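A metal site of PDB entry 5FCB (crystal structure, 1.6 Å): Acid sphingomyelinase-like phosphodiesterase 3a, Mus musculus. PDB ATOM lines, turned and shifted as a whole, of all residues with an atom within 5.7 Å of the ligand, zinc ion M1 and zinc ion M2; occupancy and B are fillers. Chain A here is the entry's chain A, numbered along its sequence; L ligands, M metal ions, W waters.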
ATOM      1  N   ASP A  30      -7.027   3.320  13.528  1.00  0.00           N
ATOM      2  CA  ASP A  30      -5.811   3.186  14.334  1.00  0.00           C
ATOM      3  C   ASP A  30      -5.226   4.550  14.697  1.00  0.00           C
ATOM      4  O   ASP A  30      -4.077   4.868  14.404  1.00  0.00           O
ATOM      5  CB  ASP A  30      -4.793   2.291  13.608  1.00  0.00           C
ATOM      6  CG  ASP A  30      -5.261   0.838  13.547  1.00  0.00           C
ATOM      7  OD1 ASP A  30      -5.890   0.462  12.541  1.00  0.00           O
ATOM      8  OD2 ASP A  30      -5.021   0.119  14.542  1.00  0.00           O
ATOM      9  N   HIS A  32      -4.787   5.756  17.823  1.00  0.00           N
ATOM     10  CA  HIS A  32      -3.828   5.542  18.915  1.00  0.00           C
ATOM     11  C   HIS A  32      -3.331   6.876  19.493  1.00  0.00           C
ATOM     12  O   HIS A  32      -2.141   7.191  19.442  1.00  0.00           O
ATOM     13  CB  HIS A  32      -2.642   4.686  18.459  1.00  0.00           C
ATOM     14  CG  HIS A  32      -2.989   3.249  18.168  1.00  0.00           C
ATOM     15  ND1 HIS A  32      -3.347   2.348  19.151  1.00  0.00           N
ATOM     16  CD2 HIS A  32      -2.978   2.565  17.002  1.00  0.00           C
ATOM     17  CE1 HIS A  32      -3.557   1.169  18.596  1.00  0.00           C
ATOM     18  NE2 HIS A  32      -3.339   1.273  17.295  1.00  0.00           N
ATOM     19  N   GLY A  94     -11.231   1.496  14.611  1.00  0.00           N
ATOM     20  CA  GLY A  94     -10.841   1.167  15.970  1.00  0.00           C
ATOM     21  C   GLY A  94      -9.397   1.508  16.321  1.00  0.00           C
ATOM     22  O   GLY A  94      -8.644   2.087  15.542  1.00  0.00           O
ATOM     23  N   ASP A  95      -9.066   1.132  17.576  1.00  0.00           N
ATOM     24  CA  ASP A  95      -7.733   1.235  18.191  1.00  0.00           C
ATOM     25  C   ASP A  95      -7.376   2.660  18.572  1.00  0.00           C
ATOM     26  O   ASP A  95      -6.509   3.294  17.943  1.00  0.00           O
ATOM     27  CB  ASP A  95      -6.657   0.615  17.280  1.00  0.00           C
ATOM     28  CG  ASP A  95      -6.174  -0.743  17.793  1.00  0.00           C
ATOM     29  OD1 ASP A  95      -6.838  -1.314  18.679  1.00  0.00           O
ATOM     30  OD2 ASP A  95      -5.141  -1.248  17.283  1.00  0.00           O
ATOM     31  N   HIS A  99      -0.191   2.441  22.758  1.00  0.00           N
ATOM     32  CA  HIS A  99       0.572   1.238  23.093  1.00  0.00           C
ATOM     33  C   HIS A  99       1.426   1.512  24.319  1.00  0.00           C
ATOM     34  O   HIS A  99       2.583   1.963  24.227  1.00  0.00           O
ATOM     35  CB  HIS A  99       1.461   0.811  21.919  1.00  0.00           C
ATOM     36  CG  HIS A  99       0.714   0.502  20.649  1.00  0.00           C
ATOM     37  ND1 HIS A  99       0.256   1.471  19.792  1.00  0.00           N
ATOM     38  CD2 HIS A  99       0.383  -0.686  20.094  1.00  0.00           C
ATOM     39  CE1 HIS A  99      -0.333   0.903  18.756  1.00  0.00           C
ATOM     40  NE2 HIS A  99      -0.269  -0.412  18.910  1.00  0.00           N
ATOM     41  N   GLY A 135     -11.367  -1.876  18.190  1.00  0.00           N
ATOM     42  CA  GLY A 135     -10.075  -2.506  17.999  1.00  0.00           C
ATOM     43  C   GLY A 135      -9.625  -3.237  19.262  1.00  0.00           C
ATOM     44  O   GLY A 135     -10.248  -3.181  20.320  1.00  0.00           O
ATOM     45  N   ASN A 136      -8.503  -3.959  19.132  1.00  0.00           N
ATOM     46  CA  ASN A 136      -8.045  -4.781  20.252  1.00  0.00           C
ATOM     47  C   ASN A 136      -7.516  -3.942  21.409  1.00  0.00           C
ATOM     48  O   ASN A 136      -7.523  -4.411  22.551  1.00  0.00           O
ATOM     49  CB  ASN A 136      -7.002  -5.787  19.777  1.00  0.00           C
ATOM     50  CG  ASN A 136      -5.847  -5.142  19.062  1.00  0.00           C
ATOM     51  OD1 ASN A 136      -6.018  -4.529  18.008  1.00  0.00           O
ATOM     52  ND2 ASN A 136      -4.648  -5.297  19.619  1.00  0.00           N
ATOM     53  N   HIS A 137      -7.064  -2.717  21.164  1.00  0.00           N
ATOM     54  CA  HIS A 137      -6.677  -1.822  22.241  1.00  0.00           C
ATOM     55  C   HIS A 137      -7.850  -1.063  22.844  1.00  0.00           C
ATOM     56  O   HIS A 137      -7.646  -0.348  23.835  1.00  0.00           O
ATOM     57  CB  HIS A 137      -5.645  -0.815  21.740  1.00  0.00           C
ATOM     58  CG  HIS A 137      -4.321  -1.433  21.460  1.00  0.00           C
ATOM     59  ND1 HIS A 137      -3.317  -1.531  22.410  1.00  0.00           N
ATOM     60  CD2 HIS A 137      -3.837  -2.051  20.349  1.00  0.00           C
ATOM     61  CE1 HIS A 137      -2.272  -2.141  21.883  1.00  0.00           C
ATOM     62  NE2 HIS A 137      -2.561  -2.469  20.639  1.00  0.00           N
ATOM     63  N   GLN A 142      -5.824  -4.765  27.229  1.00  0.00           N
ATOM     64  CA  GLN A 142      -5.903  -4.863  25.779  1.00  0.00           C
ATOM     65  C   GLN A 142      -6.093  -6.313  25.364  1.00  0.00           C
ATOM     66  O   GLN A 142      -5.618  -7.248  26.022  1.00  0.00           O
ATOM     67  CB  GLN A 142      -4.643  -4.294  25.130  1.00  0.00           C
ATOM     68  CG  GLN A 142      -3.357  -5.060  25.370  1.00  0.00           C
ATOM     69  CD  GLN A 142      -2.216  -4.556  24.483  1.00  0.00           C
ATOM     70  OE1 GLN A 142      -1.524  -3.600  24.815  1.00  0.00           O
ATOM     71  NE2 GLN A 142      -2.022  -5.219  23.350  1.00  0.00           N
ATOM     72  N   ASP A 143      -6.783  -6.498  24.244  1.00  0.00           N
ATOM     73  CA  ASP A 143      -6.997  -7.756  23.550  1.00  0.00           C
ATOM     74  C   ASP A 143      -8.018  -8.650  24.241  1.00  0.00           C
ATOM     75  O   ASP A 143      -8.450  -9.631  23.631  1.00  0.00           O
ATOM     76  CB  ASP A 143      -5.687  -8.556  23.373  1.00  0.00           C
ATOM     77  CG  ASP A 143      -4.562  -7.725  22.787  1.00  0.00           C
ATOM     78  OD1 ASP A 143      -4.851  -6.787  22.019  1.00  0.00           O
ATOM     79  OD2 ASP A 143      -3.385  -8.011  23.095  1.00  0.00           O
ATOM     80  N   TYR A 199      -8.929 -12.823  17.780  1.00  0.00           N
ATOM     81  CA  TYR A 199      -7.528 -12.429  17.761  1.00  0.00           C
ATOM     82  C   TYR A 199      -6.746 -13.272  18.770  1.00  0.00           C
ATOM     83  O   TYR A 199      -7.193 -13.472  19.906  1.00  0.00           O
ATOM     84  CB  TYR A 199      -7.461 -10.931  18.057  1.00  0.00           C
ATOM     85  CG  TYR A 199      -6.101 -10.296  18.048  1.00  0.00           C
ATOM     86  CD1 TYR A 199      -5.231 -10.454  16.974  1.00  0.00           C
ATOM     87  CD2 TYR A 199      -5.723  -9.462  19.093  1.00  0.00           C
ATOM     88  CE1 TYR A 199      -4.003  -9.825  16.974  1.00  0.00           C
ATOM     89  CE2 TYR A 199      -4.502  -8.843  19.099  1.00  0.00           C
ATOM     90  CZ  TYR A 199      -3.636  -9.028  18.042  1.00  0.00           C
ATOM     91  OH  TYR A 199      -2.418  -8.390  18.059  1.00  0.00           O
ATOM     92  N   HIS A 237     -11.789  -4.410  12.778  1.00  0.00           N
ATOM     93  CA  HIS A 237     -10.420  -4.020  13.104  1.00  0.00           C
ATOM     94  C   HIS A 237      -9.403  -5.030  12.558  1.00  0.00           C
ATOM     95  O   HIS A 237      -8.665  -4.725  11.610  1.00  0.00           O
ATOM     96  CB  HIS A 237     -10.253  -3.876  14.624  1.00  0.00           C
ATOM     97  CG  HIS A 237      -8.906  -3.366  14.992  1.00  0.00           C
ATOM     98  ND1 HIS A 237      -8.470  -2.111  14.631  1.00  0.00           N
ATOM     99  CD2 HIS A 237      -7.861  -3.959  15.618  1.00  0.00           C
ATOM    100  CE1 HIS A 237      -7.220  -1.947  15.036  1.00  0.00           C
ATOM    101  NE2 HIS A 237      -6.826  -3.049  15.642  1.00  0.00           N
ATOM    102  N   VAL A 238      -9.322  -6.202  13.168  1.00  0.00           N
ATOM    103  CA  VAL A 238      -8.358  -7.215  12.716  1.00  0.00           C
ATOM    104  C   VAL A 238      -8.863  -7.841  11.424  1.00  0.00           C
ATOM    105  O   VAL A 238     -10.046  -8.237  11.349  1.00  0.00           O
ATOM    106  CB  VAL A 238      -8.128  -8.284  13.778  1.00  0.00           C
ATOM    107  CG1 VAL A 238      -6.993  -9.228  13.340  1.00  0.00           C
ATOM    108  CG2 VAL A 238      -7.821  -7.668  15.136  1.00  0.00           C
ATOM    109  N   TYR A 245       3.790  -9.885   6.084  1.00  0.00           N
ATOM    110  CA  TYR A 245       5.191  -9.718   6.448  1.00  0.00           C
ATOM    111  C   TYR A 245       5.753 -10.923   7.201  1.00  0.00           C
ATOM    112  O   TYR A 245       6.912 -10.904   7.609  1.00  0.00           O
ATOM    113  CB  TYR A 245       5.380  -8.466   7.311  1.00  0.00           C
ATOM    114  CG  TYR A 245       4.553  -8.477   8.578  1.00  0.00           C
ATOM    115  CD1 TYR A 245       3.287  -7.937   8.602  1.00  0.00           C
ATOM    116  CD2 TYR A 245       5.045  -9.061   9.749  1.00  0.00           C
ATOM    117  CE1 TYR A 245       2.522  -7.946   9.752  1.00  0.00           C
ATOM    118  CE2 TYR A 245       4.272  -9.074  10.914  1.00  0.00           C
ATOM    119  CZ  TYR A 245       3.010  -8.518  10.904  1.00  0.00           C
ATOM    120  OH  TYR A 245       2.230  -8.515  12.023  1.00  0.00           O
ATOM    121  N   HIS A 278      -5.851  -2.369  11.867  1.00  0.00           N
ATOM    122  CA  HIS A 278      -4.996  -3.176  12.750  1.00  0.00           C
ATOM    123  C   HIS A 278      -3.543  -3.322  12.295  1.00  0.00           C
ATOM    124  O   HIS A 278      -2.632  -3.227  13.128  1.00  0.00           O
ATOM    125  CB  HIS A 278      -5.617  -4.570  12.975  1.00  0.00           C
ATOM    126  CG  HIS A 278      -4.786  -5.459  13.837  1.00  0.00           C
ATOM    127  ND1 HIS A 278      -4.599  -5.236  15.190  1.00  0.00           N
ATOM    128  CD2 HIS A 278      -4.077  -6.564  13.537  1.00  0.00           C
ATOM    129  CE1 HIS A 278      -3.808  -6.180  15.682  1.00  0.00           C
ATOM    130  NE2 HIS A 278      -3.477  -6.990  14.697  1.00  0.00           N
ATOM    131  N   THR A 279      -3.289  -3.573  10.997  1.00  0.00           N
ATOM    132  CA  THR A 279      -1.910  -3.793  10.573  1.00  0.00           C
ATOM    133  C   THR A 279      -1.124  -2.515  10.419  1.00  0.00           C
ATOM    134  O   THR A 279       0.112  -2.566  10.331  1.00  0.00           O
ATOM    135  CB  THR A 279      -1.834  -4.513   9.231  1.00  0.00           C
ATOM    136  OG1 THR A 279      -2.276  -3.630   8.216  1.00  0.00           O
ATOM    137  CG2 THR A 279      -2.687  -5.774   9.252  1.00  0.00           C
ATOM    138  N   HIS A 280      -1.800  -1.371  10.352  1.00  0.00           N
ATOM    139  CA  HIS A 280      -1.177  -0.070  10.151  1.00  0.00           C
ATOM    140  C   HIS A 280      -0.483   0.050   8.807  1.00  0.00           C
ATOM    141  O   HIS A 280       0.393   0.903   8.621  1.00  0.00           O
ATOM    142  CB  HIS A 280      -0.175   0.241  11.279  1.00  0.00           C
ATOM    143  CG  HIS A 280      -0.775   0.357  12.644  1.00  0.00           C
ATOM    144  ND1 HIS A 280      -0.128   0.988  13.679  1.00  0.00           N
ATOM    145  CD2 HIS A 280      -1.948  -0.097  13.153  1.00  0.00           C
ATOM    146  CE1 HIS A 280      -0.872   0.914  14.777  1.00  0.00           C
ATOM    147  NE2 HIS A 280      -1.989   0.271  14.483  1.00  0.00           N
ATOM    148  N   ARG A 281      -0.865  -0.781   7.844  1.00  0.00           N
ATOM    149  CA  ARG A 281      -0.278  -0.781   6.511  1.00  0.00           C
ATOM    150  C   ARG A 281      -1.371  -0.691   5.454  1.00  0.00           C
ATOM    151  O   ARG A 281      -2.541  -0.970   5.721  1.00  0.00           O
ATOM    152  CB  ARG A 281       0.555  -2.048   6.285  1.00  0.00           C
ATOM    153  CG  ARG A 281       1.662  -2.259   7.301  1.00  0.00           C
ATOM    154  CD  ARG A 281       2.810  -1.304   7.064  1.00  0.00           C
ATOM    155  NE  ARG A 281       3.881  -1.513   8.041  1.00  0.00           N
ATOM    156  CZ  ARG A 281       4.013  -0.837   9.173  1.00  0.00           C
ATOM    157  NH1 ARG A 281       3.170   0.134   9.492  1.00  0.00           N
ATOM    158  NH2 ARG A 281       5.013  -1.106   9.994  1.00  0.00           N
ATOM    159  N   THR A 305      -1.533   6.797  13.387  1.00  0.00           N
ATOM    160  CA  THR A 305      -0.286   6.733  14.138  1.00  0.00           C
ATOM    161  C   THR A 305       0.855   6.206  13.267  1.00  0.00           C
ATOM    162  O   THR A 305       0.641   5.315  12.423  1.00  0.00           O
ATOM    163  CB  THR A 305      -0.422   5.859  15.389  1.00  0.00           C
ATOM    164  OG1 THR A 305       0.805   5.888  16.139  1.00  0.00           O
ATOM    165  CG2 THR A 305      -0.728   4.399  15.044  1.00  0.00           C
ATOM    166  N   GLN A 312      11.859  -2.583  14.571  1.00  0.00           N
ATOM    167  CA  GLN A 312      11.364  -2.487  13.200  1.00  0.00           C
ATOM    168  C   GLN A 312      12.166  -1.479  12.400  1.00  0.00           C
ATOM    169  O   GLN A 312      12.484  -0.397  12.892  1.00  0.00           O
ATOM    170  CB  GLN A 312       9.884  -2.068  13.183  1.00  0.00           C
ATOM    171  CG  GLN A 312       8.949  -3.116  13.751  1.00  0.00           C
ATOM    172  CD  GLN A 312       7.523  -2.594  13.909  1.00  0.00           C
ATOM    173  OE1 GLN A 312       7.081  -2.307  15.019  1.00  0.00           O
ATOM    174  NE2 GLN A 312       6.804  -2.453  12.793  1.00  0.00           N
ATOM    175  N   TYR A 395       2.766   0.346   0.642  1.00  0.00           N
ATOM    176  CA  TYR A 395       2.493  -0.494   1.816  1.00  0.00           C
ATOM    177  C   TYR A 395       2.851   0.237   3.104  1.00  0.00           C
ATOM    178  O   TYR A 395       2.088   0.207   4.089  1.00  0.00           O
ATOM    179  CB  TYR A 395       3.272  -1.822   1.650  1.00  0.00           C
ATOM    180  CG  TYR A 395       3.259  -2.773   2.826  1.00  0.00           C
ATOM    181  CD1 TYR A 395       2.110  -3.480   3.200  1.00  0.00           C
ATOM    182  CD2 TYR A 395       4.429  -3.004   3.560  1.00  0.00           C
ATOM    183  CE1 TYR A 395       2.113  -4.354   4.280  1.00  0.00           C
ATOM    184  CE2 TYR A 395       4.442  -3.876   4.640  1.00  0.00           C
ATOM    185  CZ  TYR A 395       3.295  -4.550   5.006  1.00  0.00           C
ATOM    186  OH  TYR A 395       3.335  -5.402   6.085  1.00  0.00           O
HETATM  187  P1  LIG L   1      -1.762  -3.365  17.658  1.00  0.00           P
HETATM  188  O1  LIG L   1      -1.002  -3.575  18.950  1.00  0.00           O
HETATM  189  O2  LIG L   1      -1.581  -1.961  17.105  1.00  0.00           O
HETATM  190  O3  LIG L   1      -3.194  -3.859  17.667  1.00  0.00           O
HETATM  191  O4  LIG L   1      -0.983  -4.345  16.676  1.00  0.00           O
HETATM  192  C1  LIG L   1       0.430  -4.368  16.687  1.00  0.00           C
HETATM  193  C2  LIG L   1       1.012  -5.682  17.153  1.00  0.00           C
HETATM  194  O5  LIG L   1       1.495  -6.406  15.992  1.00  0.00           O
HETATM  195  C3  LIG L   1       2.210  -5.550  18.074  1.00  0.00           C
HETATM  196  O6  LIG L   1       2.361  -6.745  18.844  1.00  0.00           O
HETATM  197  C4  LIG L   1       3.352  -5.421  17.081  1.00  0.00           C
HETATM  198  O7  LIG L   1       4.635  -5.735  17.603  1.00  0.00           O
HETATM  199  C5  LIG L   1       2.924  -6.375  15.968  1.00  0.00           C
HETATM  200  N1  LIG L   1       3.326  -5.957  14.620  1.00  0.00           N
HETATM  201  C6  LIG L   1       2.523  -5.287  13.768  1.00  0.00           C
HETATM  202  N2  LIG L   1       3.127  -5.023  12.588  1.00  0.00           N
HETATM  203  C7  LIG L   1       4.366  -5.540  12.667  1.00  0.00           C
HETATM  204  C8  LIG L   1       5.506  -5.612  11.743  1.00  0.00           C
HETATM  205  N3  LIG L   1       5.393  -5.044  10.520  1.00  0.00           N
HETATM  206  N4  LIG L   1       6.623  -6.235  12.179  1.00  0.00           N
HETATM  207  C9  LIG L   1       6.701  -6.781  13.411  1.00  0.00           C
HETATM  208  N5  LIG L   1       5.680  -6.751  14.296  1.00  0.00           N
HETATM  209  C10 LIG L   1       4.500  -6.165  13.999  1.00  0.00           C
HETATM  210 ZN    ZN M   1      -4.962  -3.455  16.492  1.00  0.00          ZN
HETATM  211 ZN    ZN M   2      -3.545  -0.290  15.906  1.00  0.00          ZN
HETATM  212  O   HOH W   1      -3.428  -2.291  15.514  1.00  0.00           O
HETATM  213  O   HOH W   2       7.457  -2.486   9.954  1.00  0.00           O
HETATM  214  O   HOH W   3       0.023  -4.578  21.357  1.00  0.00           O
HETATM  215  O   HOH W   4      -0.588  -5.001  13.780  1.00  0.00           O
HETATM  216  O   HOH W   5       8.344  -6.840   9.313  1.00  0.00           O
HETATM  217  O   HOH W   6       1.531  -4.830   9.966  1.00  0.00           O
HETATM  218  O   HOH W   7       5.027  -4.188   8.006  1.00  0.00           O
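An oxygen (O2) of the ligand lies close to a ring nitrogen (NE2) of His 280 (3.5 Å). NE2 of His 137 is in hydrogen-bond range of O1 of the ligand, 2.6 Å away. An oxygen (O2) of the ligand is in hydrogen-bond range of a ring nitrogen (NE2) of His 99 (2.7 Å).
The backbone NH of His 278 sits at hydrogen-bond distance from the side-chain carboxylate of Asp 30 (2.9 Å). O of Asp 30 is in hydrogen-bond range of N of Thr 305, at 3.4 Å. The backbone carbonyl oxygen of Gly 94 sits at hydrogen-bond distance from the backbone NH of Asp 30 (2.9 Å). The backbone carbonyl oxygen (O) of Asn 136 sits at hydrogen-bond distance from the backbone NH (N) of Asp 143 (2.8 Å). The backbone NH of His 137 lies within hydrogen-bond range of the side-chain carboxylate of Asp 95, 2.9 Å away. The backbone NH of Arg 281 lies close to the side-chain hydroxyl of Thr 279 (3.2 Å).
Residues that only touch the ligand: Tyr 245, Arg 281 and Gln 312. Of the 21 residues printed, 10 come within 4 Å of the ligand. Along chain A the residues within 4 Å of the ligand span positions 32 to 312. The nearest printed residue that does not touch the ligand is His 237 (4.2 Å).
Of the 21 residues printed, 4 come within 4 Å of zinc ion M1.
Four residues have an atom within 4 Å of zinc ion M2: Asp 30, His 32, Asp 95 and His 280.
Zinc ion M1 is bound by NE2 of His 237 (2.1 Å). Zinc ion M1 is bound by OD1 of Asn 136 (2.1 Å). Zinc ion M1 is bound by water W1, at 2.2 Å. Zinc ion M1 is bound by O3 of the ligand, at 2.2 Å. ND1 of His 278 binds zinc ion M1. The side-chain carboxylate (OD2) of Asp 95 is bound to zinc ion M1 (2.4 Å).
Water W1 binds zinc ion M2, at 2.0 Å. OD2 of Asp 30 is bound to zinc ion M2. NE2 of His 32 is bound to zinc ion M2, 2.1 Å away. Zinc ion M2 is bound by a ring nitrogen (NE2) of His 280, 2.2 Å away. OD2 of Asp 95 binds zinc ion M2, at 2.3 Å. Zinc ion M2 has five donor atoms within binding distance. Slightly farther from zinc ion M2 lies an oxygen (O2) of the ligand (2.8 Å).
Water W1 bridges an oxygen (O2) of the ligand (2.5 Å) and the backbone carbonyl oxygen (O) of His 278 (2.7 Å). Water W7 lies within hydrogen-bond range of a nitrogen (N3) of the ligand (2.7 Å), the side-chain hydroxyl of Tyr 395 (2.8 Å) and the guanidinium group of Arg 281 (2.9 Å). Water W3 lies within hydrogen-bond range of an oxygen (O1) of the ligand (2.8 Å), the side-chain amide nitrogen of Gln 142 (2.9 Å) and a ring nitrogen (NE2) of His 137 (3.4 Å). Water W4 bridges the backbone carbonyl oxygen (O) of His 278 (2.8 Å) and an oxygen (O4) of the ligand (3.0 Å). Water W6 lies within hydrogen-bond range of O of Thr 279 (2.7 Å) and N2 of the ligand (3.1 Å).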
